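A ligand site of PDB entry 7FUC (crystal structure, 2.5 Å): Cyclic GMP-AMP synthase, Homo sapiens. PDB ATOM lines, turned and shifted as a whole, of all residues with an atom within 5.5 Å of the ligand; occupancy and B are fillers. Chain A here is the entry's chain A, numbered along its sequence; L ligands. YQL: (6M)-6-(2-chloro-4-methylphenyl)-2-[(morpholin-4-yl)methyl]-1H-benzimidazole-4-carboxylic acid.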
ATOM      1  N   LYS A  59      -4.855  17.253 -13.706  1.00  0.00           N
ATOM      2  CA  LYS A  59      -6.083  17.470 -14.488  1.00  0.00           C
ATOM      3  C   LYS A  59      -5.925  18.723 -15.360  1.00  0.00           C
ATOM      4  O   LYS A  59      -5.244  19.666 -14.951  1.00  0.00           O
ATOM      5  CB  LYS A  59      -7.316  17.575 -13.576  1.00  0.00           C
ATOM      6  CG  LYS A  59      -8.586  17.081 -14.246  1.00  0.00           C
ATOM      7  CD  LYS A  59      -9.786  17.077 -13.302  1.00  0.00           C
ATOM      8  CE  LYS A  59     -10.785  16.019 -13.697  1.00  0.00           C
ATOM      9  NZ  LYS A  59     -12.051  16.113 -12.917  1.00  0.00           N
ATOM     10  N   ASP A  67      -5.113  21.816 -13.194  1.00  0.00           N
ATOM     11  CA  ASP A  67      -5.762  21.686 -11.901  1.00  0.00           C
ATOM     12  C   ASP A  67      -5.220  20.480 -11.147  1.00  0.00           C
ATOM     13  O   ASP A  67      -5.276  19.364 -11.652  1.00  0.00           O
ATOM     14  CB  ASP A  67      -7.293  21.604 -12.043  1.00  0.00           C
ATOM     15  CG  ASP A  67      -7.957  22.823 -12.675  1.00  0.00           C
ATOM     16  OD1 ASP A  67      -7.481  23.959 -12.443  1.00  0.00           O
ATOM     17  OD2 ASP A  67      -8.949  22.637 -13.405  1.00  0.00           O
ATOM     18  N   LEU A 178     -26.272  11.857 -10.077  1.00  0.00           N
ATOM     19  CA  LEU A 178     -25.552  10.811 -10.820  1.00  0.00           C
ATOM     20  C   LEU A 178     -26.580   9.810 -11.412  1.00  0.00           C
ATOM     21  O   LEU A 178     -26.619   8.651 -11.019  1.00  0.00           O
ATOM     22  CB  LEU A 178     -24.495  10.152  -9.908  1.00  0.00           C
ATOM     23  CG  LEU A 178     -23.497   9.160 -10.520  1.00  0.00           C
ATOM     24  CD1 LEU A 178     -22.508   9.857 -11.442  1.00  0.00           C
ATOM     25  CD2 LEU A 178     -22.778   8.388  -9.440  1.00  0.00           C
ATOM     26  N   LYS A 202     -14.804  26.351  -1.650  1.00  0.00           N
ATOM     27  CA  LYS A 202     -15.471  27.351  -2.480  1.00  0.00           C
ATOM     28  C   LYS A 202     -16.487  28.082  -1.596  1.00  0.00           C
ATOM     29  O   LYS A 202     -17.249  27.438  -0.877  1.00  0.00           O
ATOM     30  CB  LYS A 202     -16.126  26.730  -3.737  1.00  0.00           C
ATOM     31  CG  LYS A 202     -16.692  27.786  -4.692  1.00  0.00           C
ATOM     32  CD  LYS A 202     -16.850  27.285  -6.109  1.00  0.00           C
ATOM     33  CE  LYS A 202     -17.325  28.401  -7.018  1.00  0.00           C
ATOM     34  NZ  LYS A 202     -17.379  27.964  -8.433  1.00  0.00           N
ATOM     35  N   ARG A 216     -17.782  23.466  -0.483  1.00  0.00           N
ATOM     36  CA  ARG A 216     -18.586  22.958  -1.594  1.00  0.00           C
ATOM     37  C   ARG A 216     -18.332  21.471  -1.824  1.00  0.00           C
ATOM     38  O   ARG A 216     -17.191  21.022  -1.706  1.00  0.00           O
ATOM     39  CB  ARG A 216     -18.281  23.758  -2.863  1.00  0.00           C
ATOM     40  CG  ARG A 216     -19.336  23.641  -3.958  1.00  0.00           C
ATOM     41  CD  ARG A 216     -18.782  24.126  -5.282  1.00  0.00           C
ATOM     42  NE  ARG A 216     -19.140  23.228  -6.377  1.00  0.00           N
ATOM     43  CZ  ARG A 216     -18.393  22.199  -6.796  1.00  0.00           C
ATOM     44  NH1 ARG A 216     -17.233  21.932  -6.217  1.00  0.00           N
ATOM     45  NH2 ARG A 216     -18.812  21.437  -7.803  1.00  0.00           N
ATOM     46  N   LEU A 217     -19.391  20.708  -2.186  1.00  0.00           N
ATOM     47  CA  LEU A 217     -19.313  19.271  -2.475  1.00  0.00           C
ATOM     48  C   LEU A 217     -18.642  19.036  -3.832  1.00  0.00           C
ATOM     49  O   LEU A 217     -19.152  19.497  -4.871  1.00  0.00           O
ATOM     50  CB  LEU A 217     -20.703  18.605  -2.460  1.00  0.00           C
ATOM     51  CG  LEU A 217     -21.393  18.326  -1.122  1.00  0.00           C
ATOM     52  CD1 LEU A 217     -22.595  17.430  -1.329  1.00  0.00           C
ATOM     53  CD2 LEU A 217     -20.455  17.663  -0.113  1.00  0.00           C
ATOM     54  N   SER A 218     -17.515  18.326  -3.832  1.00  0.00           N
ATOM     55  CA  SER A 218     -16.782  18.028  -5.059  1.00  0.00           C
ATOM     56  C   SER A 218     -16.736  16.539  -5.384  1.00  0.00           C
ATOM     57  O   SER A 218     -16.438  15.715  -4.511  1.00  0.00           O
ATOM     58  CB  SER A 218     -15.385  18.631  -5.016  1.00  0.00           C
ATOM     59  OG  SER A 218     -14.800  18.588  -6.307  1.00  0.00           O
ATOM     60  N   PHE A 219     -17.062  16.194  -6.635  1.00  0.00           N
ATOM     61  CA  PHE A 219     -17.105  14.836  -7.147  1.00  0.00           C
ATOM     62  C   PHE A 219     -16.289  14.723  -8.436  1.00  0.00           C
ATOM     63  O   PHE A 219     -16.568  13.889  -9.301  1.00  0.00           O
ATOM     64  CB  PHE A 219     -18.567  14.389  -7.335  1.00  0.00           C
ATOM     65  CG  PHE A 219     -19.388  14.390  -6.073  1.00  0.00           C
ATOM     66  CD1 PHE A 219     -19.396  13.288  -5.230  1.00  0.00           C
ATOM     67  CD2 PHE A 219     -20.165  15.497  -5.722  1.00  0.00           C
ATOM     68  CE1 PHE A 219     -20.155  13.278  -4.065  1.00  0.00           C
ATOM     69  CE2 PHE A 219     -20.921  15.497  -4.559  1.00  0.00           C
ATOM     70  CZ  PHE A 219     -20.910  14.397  -3.728  1.00  0.00           C
ATOM     71  N   SER A 220     -15.248  15.574  -8.527  1.00  0.00           N
ATOM     72  CA  SER A 220     -14.274  15.700  -9.608  1.00  0.00           C
ATOM     73  C   SER A 220     -13.648  14.344  -9.982  1.00  0.00           C
ATOM     74  O   SER A 220     -13.572  13.999 -11.165  1.00  0.00           O
ATOM     75  CB  SER A 220     -13.201  16.707  -9.198  1.00  0.00           C
ATOM     76  OG  SER A 220     -12.267  16.909 -10.235  1.00  0.00           O
ATOM     77  N   ILE A 222     -14.798  11.386  -9.944  1.00  0.00           N
ATOM     78  CA  ILE A 222     -15.715  10.452 -10.609  1.00  0.00           C
ATOM     79  C   ILE A 222     -15.620  10.518 -12.156  1.00  0.00           C
ATOM     80  O   ILE A 222     -15.867   9.519 -12.820  1.00  0.00           O
ATOM     81  CB  ILE A 222     -17.182  10.645 -10.075  1.00  0.00           C
ATOM     82  CG1 ILE A 222     -17.272  10.435  -8.536  1.00  0.00           C
ATOM     83  CG2 ILE A 222     -18.234   9.774 -10.825  1.00  0.00           C
ATOM     84  CD1 ILE A 222     -16.800   9.067  -7.965  1.00  0.00           C
ATOM     85  N   GLU A 223     -15.253  11.686 -12.718  1.00  0.00           N
ATOM     86  CA  GLU A 223     -15.121  11.894 -14.165  1.00  0.00           C
ATOM     87  C   GLU A 223     -14.219  10.862 -14.844  1.00  0.00           C
ATOM     88  O   GLU A 223     -14.627  10.299 -15.857  1.00  0.00           O
ATOM     89  CB  GLU A 223     -14.636  13.315 -14.425  1.00  0.00           C
ATOM     90  CG  GLU A 223     -14.534  13.700 -15.887  1.00  0.00           C
ATOM     91  CD  GLU A 223     -13.884  15.042 -16.128  1.00  0.00           C
ATOM     92  OE1 GLU A 223     -13.732  15.831 -15.170  1.00  0.00           O
ATOM     93  OE2 GLU A 223     -13.530  15.302 -17.303  1.00  0.00           O
ATOM     94  N   ILE A 226     -16.001   7.374 -15.046  1.00  0.00           N
ATOM     95  CA  ILE A 226     -17.011   7.315 -16.113  1.00  0.00           C
ATOM     96  C   ILE A 226     -16.366   7.464 -17.510  1.00  0.00           C
ATOM     97  O   ILE A 226     -16.648   6.634 -18.362  1.00  0.00           O
ATOM     98  CB  ILE A 226     -18.174   8.302 -15.858  1.00  0.00           C
ATOM     99  CG1 ILE A 226     -18.965   7.852 -14.601  1.00  0.00           C
ATOM    100  CG2 ILE A 226     -19.092   8.413 -17.085  1.00  0.00           C
ATOM    101  CD1 ILE A 226     -20.221   8.626 -14.194  1.00  0.00           C
ATOM    102  N   SER A 274     -16.610  27.906 -17.434  1.00  0.00           N
ATOM    103  CA  SER A 274     -15.482  26.971 -17.388  1.00  0.00           C
ATOM    104  C   SER A 274     -15.837  25.682 -18.099  1.00  0.00           C
ATOM    105  O   SER A 274     -17.011  25.451 -18.406  1.00  0.00           O
ATOM    106  CB  SER A 274     -15.093  26.669 -15.940  1.00  0.00           C
ATOM    107  OG  SER A 274     -16.184  26.138 -15.211  1.00  0.00           O
ATOM    108  N   TYR A 276     -16.068  22.956 -16.841  1.00  0.00           N
ATOM    109  CA  TYR A 276     -16.953  22.302 -15.880  1.00  0.00           C
ATOM    110  C   TYR A 276     -18.428  22.355 -16.323  1.00  0.00           C
ATOM    111  O   TYR A 276     -19.122  21.342 -16.239  1.00  0.00           O
ATOM    112  CB  TYR A 276     -16.775  22.940 -14.494  1.00  0.00           C
ATOM    113  CG  TYR A 276     -17.738  22.465 -13.424  1.00  0.00           C
ATOM    114  CD1 TYR A 276     -17.907  21.109 -13.163  1.00  0.00           C
ATOM    115  CD2 TYR A 276     -18.389  23.378 -12.610  1.00  0.00           C
ATOM    116  CE1 TYR A 276     -18.778  20.671 -12.175  1.00  0.00           C
ATOM    117  CE2 TYR A 276     -19.252  22.945 -11.593  1.00  0.00           C
ATOM    118  CZ  TYR A 276     -19.445  21.596 -11.376  1.00  0.00           C
ATOM    119  OH  TYR A 276     -20.278  21.158 -10.389  1.00  0.00           O
ATOM    120  N   LYS A 279     -18.724  20.070 -19.325  1.00  0.00           N
ATOM    121  CA  LYS A 279     -18.722  18.663 -18.884  1.00  0.00           C
ATOM    122  C   LYS A 279     -20.113  18.261 -18.401  1.00  0.00           C
ATOM    123  O   LYS A 279     -20.710  17.365 -18.995  1.00  0.00           O
ATOM    124  CB  LYS A 279     -17.666  18.402 -17.794  1.00  0.00           C
ATOM    125  CG  LYS A 279     -16.212  18.441 -18.273  1.00  0.00           C
ATOM    126  CD  LYS A 279     -15.264  18.344 -17.089  1.00  0.00           C
ATOM    127  CE  LYS A 279     -13.828  18.659 -17.431  1.00  0.00           C
ATOM    128  NZ  LYS A 279     -12.914  18.356 -16.296  1.00  0.00           N
ATOM    129  N   THR A 280     -20.655  18.986 -17.386  1.00  0.00           N
ATOM    130  CA  THR A 280     -21.999  18.777 -16.801  1.00  0.00           C
ATOM    131  C   THR A 280     -23.059  18.611 -17.889  1.00  0.00           C
ATOM    132  O   THR A 280     -23.821  17.654 -17.836  1.00  0.00           O
ATOM    133  CB  THR A 280     -22.348  19.936 -15.834  1.00  0.00           C
ATOM    134  OG1 THR A 280     -21.338  20.076 -14.831  1.00  0.00           O
ATOM    135  CG2 THR A 280     -23.682  19.728 -15.149  1.00  0.00           C
ATOM    136  N   PHE A 283     -22.508  15.245 -19.991  1.00  0.00           N
ATOM    137  CA  PHE A 283     -22.939  14.055 -19.247  1.00  0.00           C
ATOM    138  C   PHE A 283     -24.458  13.959 -19.125  1.00  0.00           C
ATOM    139  O   PHE A 283     -24.995  12.836 -19.072  1.00  0.00           O
ATOM    140  CB  PHE A 283     -22.234  13.935 -17.887  1.00  0.00           C
ATOM    141  CG  PHE A 283     -20.780  13.534 -18.013  1.00  0.00           C
ATOM    142  CD1 PHE A 283     -20.423  12.221 -18.328  1.00  0.00           C
ATOM    143  CD2 PHE A 283     -19.761  14.466 -17.847  1.00  0.00           C
ATOM    144  CE1 PHE A 283     -19.083  11.863 -18.468  1.00  0.00           C
ATOM    145  CE2 PHE A 283     -18.424  14.094 -17.961  1.00  0.00           C
ATOM    146  CZ  PHE A 283     -18.089  12.787 -18.274  1.00  0.00           C
ATOM    147  N   ASN A 322     -26.216  20.590 -11.400  1.00  0.00           N
ATOM    148  CA  ASN A 322     -24.974  19.929 -11.014  1.00  0.00           C
ATOM    149  C   ASN A 322     -25.291  18.423 -11.160  1.00  0.00           C
ATOM    150  O   ASN A 322     -26.351  17.970 -10.690  1.00  0.00           O
ATOM    151  CB  ASN A 322     -24.610  20.289  -9.564  1.00  0.00           C
ATOM    152  CG  ASN A 322     -23.306  19.727  -9.046  1.00  0.00           C
ATOM    153  OD1 ASN A 322     -23.113  18.528  -8.923  1.00  0.00           O
ATOM    154  ND2 ASN A 322     -22.398  20.605  -8.667  1.00  0.00           N
ATOM    155  N   TYR A 323     -24.442  17.691 -11.906  1.00  0.00           N
ATOM    156  CA  TYR A 323     -24.657  16.278 -12.202  1.00  0.00           C
ATOM    157  C   TYR A 323     -24.888  15.405 -10.963  1.00  0.00           C
ATOM    158  O   TYR A 323     -25.587  14.398 -11.040  1.00  0.00           O
ATOM    159  CB  TYR A 323     -23.505  15.737 -13.064  1.00  0.00           C
ATOM    160  CG  TYR A 323     -23.879  14.523 -13.884  1.00  0.00           C
ATOM    161  CD1 TYR A 323     -24.602  14.649 -15.068  1.00  0.00           C
ATOM    162  CD2 TYR A 323     -23.538  13.242 -13.473  1.00  0.00           C
ATOM    163  CE1 TYR A 323     -25.019  13.538 -15.786  1.00  0.00           C
ATOM    164  CE2 TYR A 323     -23.917  12.117 -14.201  1.00  0.00           C
ATOM    165  CZ  TYR A 323     -24.656  12.263 -15.364  1.00  0.00           C
ATOM    166  OH  TYR A 323     -25.022  11.171 -16.115  1.00  0.00           O
ATOM    167  N   PHE A 324     -24.350  15.836  -9.800  1.00  0.00           N
ATOM    168  CA  PHE A 324     -24.434  15.121  -8.520  1.00  0.00           C
ATOM    169  C   PHE A 324     -25.480  15.691  -7.585  1.00  0.00           C
ATOM    170  O   PHE A 324     -26.014  14.948  -6.765  1.00  0.00           O
ATOM    171  CB  PHE A 324     -23.063  15.104  -7.838  1.00  0.00           C
ATOM    172  CG  PHE A 324     -22.054  14.305  -8.620  1.00  0.00           C
ATOM    173  CD1 PHE A 324     -21.363  14.886  -9.681  1.00  0.00           C
ATOM    174  CD2 PHE A 324     -21.841  12.953  -8.349  1.00  0.00           C
ATOM    175  CE1 PHE A 324     -20.476  14.128 -10.448  1.00  0.00           C
ATOM    176  CE2 PHE A 324     -20.942  12.204  -9.101  1.00  0.00           C
ATOM    177  CZ  PHE A 324     -20.274  12.797 -10.148  1.00  0.00           C
HETATM  178  C10 YQL L   1     -15.952  19.019 -10.916  1.00  0.00           C
HETATM  179  C11 YQL L   1     -15.629  18.643 -12.227  1.00  0.00           C
HETATM  180  C13 YQL L   1     -16.259  17.591 -12.886  1.00  0.00           C
HETATM  181  C15 YQL L   1     -17.905  15.692 -12.870  1.00  0.00           C
HETATM  182  C16 YQL L   1     -18.889  15.807 -13.856  1.00  0.00           C
HETATM  183  C18 YQL L   1     -19.497  14.706 -14.420  1.00  0.00           C
HETATM  184  C19 YQL L   1     -19.159  13.428 -13.995  1.00  0.00           C
HETATM  185  C20 YQL L   1     -19.825  12.210 -14.588  1.00  0.00           C
HETATM  186  C21 YQL L   1     -18.207  13.297 -12.988  1.00  0.00           C
HETATM  187  C22 YQL L   1     -17.580  14.400 -12.435  1.00  0.00           C
HETATM  188  C23 YQL L   1     -17.580  17.208 -10.916  1.00  0.00           C
HETATM  189  C24 YQL L   1     -16.934  18.267 -10.255  1.00  0.00           C
HETATM  190  C25 YQL L   1     -17.419  18.580  -8.876  1.00  0.00           C
HETATM  191  C1  YQL L   1     -13.421  21.484 -11.677  1.00  0.00           C
HETATM  192  C14 YQL L   1     -17.246  16.852 -12.222  1.00  0.00           C
HETATM  193  C3  YQL L   1     -14.527  23.605 -11.283  1.00  0.00           C
HETATM  194  C4  YQL L   1     -14.858  24.630 -10.227  1.00  0.00           C
HETATM  195  C6  YQL L   1     -12.822  24.151  -9.107  1.00  0.00           C
HETATM  196  C7  YQL L   1     -12.486  23.109 -10.142  1.00  0.00           C
HETATM  197  C8  YQL L   1     -14.410  20.369 -11.592  1.00  0.00           C
HETATM  198  N12 YQL L   1     -14.679  19.551 -12.641  1.00  0.00           N
HETATM  199  N2  YQL L   1     -13.716  22.532 -10.703  1.00  0.00           N
HETATM  200  N9  YQL L   1     -15.166  20.104 -10.544  1.00  0.00           N
HETATM  201  O26 YQL L   1     -16.657  19.376  -8.178  1.00  0.00           O
HETATM  202  O27 YQL L   1     -18.479  18.119  -8.441  1.00  0.00           O
HETATM  203  O5  YQL L   1     -13.666  25.189  -9.654  1.00  0.00           O
HETATM  204 CL17 YQL L   1     -19.363  17.378 -14.437  1.00  0.00          CL
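OG of Ser 218 lies within hydrogen-bond range of O26 of the ligand, 2.8 Å away.
The backbone NH (N) of Phe 219 is in hydrogen-bond range of an oxygen (O27) of the ligand (3.0 Å).
NH2 of Arg 216 is in salt-bridge range of O26 of the ligand, 3.0 Å away.
The guanidinium group (NH2) of Arg 216 lies within hydrogen-bond range of the side-chain hydroxyl (OH) of Tyr 276, at 3.0 Å.
The side-chain hydroxyl of Thr 280 lies within hydrogen-bond range of the backbone carbonyl oxygen of Tyr 276 (2.9 Å).
The side-chain carboxylate (OE1) of Glu 223 lies within salt-bridge range of the side-chain amino group (NZ) of Lys 279, at 2.9 Å.
The side-chain amino group of Lys 59 is in salt-bridge range of the side-chain carboxylate of Glu 223 (2.8 Å).
OH of Tyr 323 lies close to O of Phe 283, at 3.4 Å.
The side-chain amide nitrogen (ND2) of Asn 322 sits at hydrogen-bond distance from the side-chain hydroxyl (OH) of Tyr 276, 2.8 Å away.
The side-chain amide oxygen (OD1) of Asn 322 sits close to the backbone NH (N) of Phe 324 (3.1 Å).
The side-chain amino group (NZ) of Lys 59 sits at hydrogen-bond distance from the side-chain hydroxyl (OG) of Ser 220 (2.8 Å).
Leu 217 touches the ligand (O to O27, 3.9 Å).
Ser 220 touches the ligand.
Ile 222 touches the ligand (C to C21, 3.9 Å).
N of Glu 223 touches C21 of the ligand (3.4 Å).
Ile 226 touches the ligand (CD1 to C20, 3.6 Å).
Tyr 276 touches the ligand (CD1 to C11, 3.5 Å).
Lys 279 touches the ligand (CB to CL17, 3.9 Å).
OG1 of Thr 280 touches CL17 of the ligand (3.4 Å).
Phe 283 touches the ligand (CD2 to C18, 3.4 Å).
CE1 of Phe 324 touches C21 of the ligand, at 3.5 Å.
Hydrophobic or aromatic side chains that line the ligand: Phe 219, Ile 226, Tyr 276, Phe 283 and Phe 324.
13 residues have an atom within 4 Å of the ligand: Arg 216, Leu 217, Ser 218, Phe 219, Ser 220, Ile 222, Glu 223, Ile 226, Tyr 276, Lys 279, Thr 280, Phe 283 and Phe 324.
The nearest printed residue that does not touch the ligand is Tyr 323 (4.01 Å).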
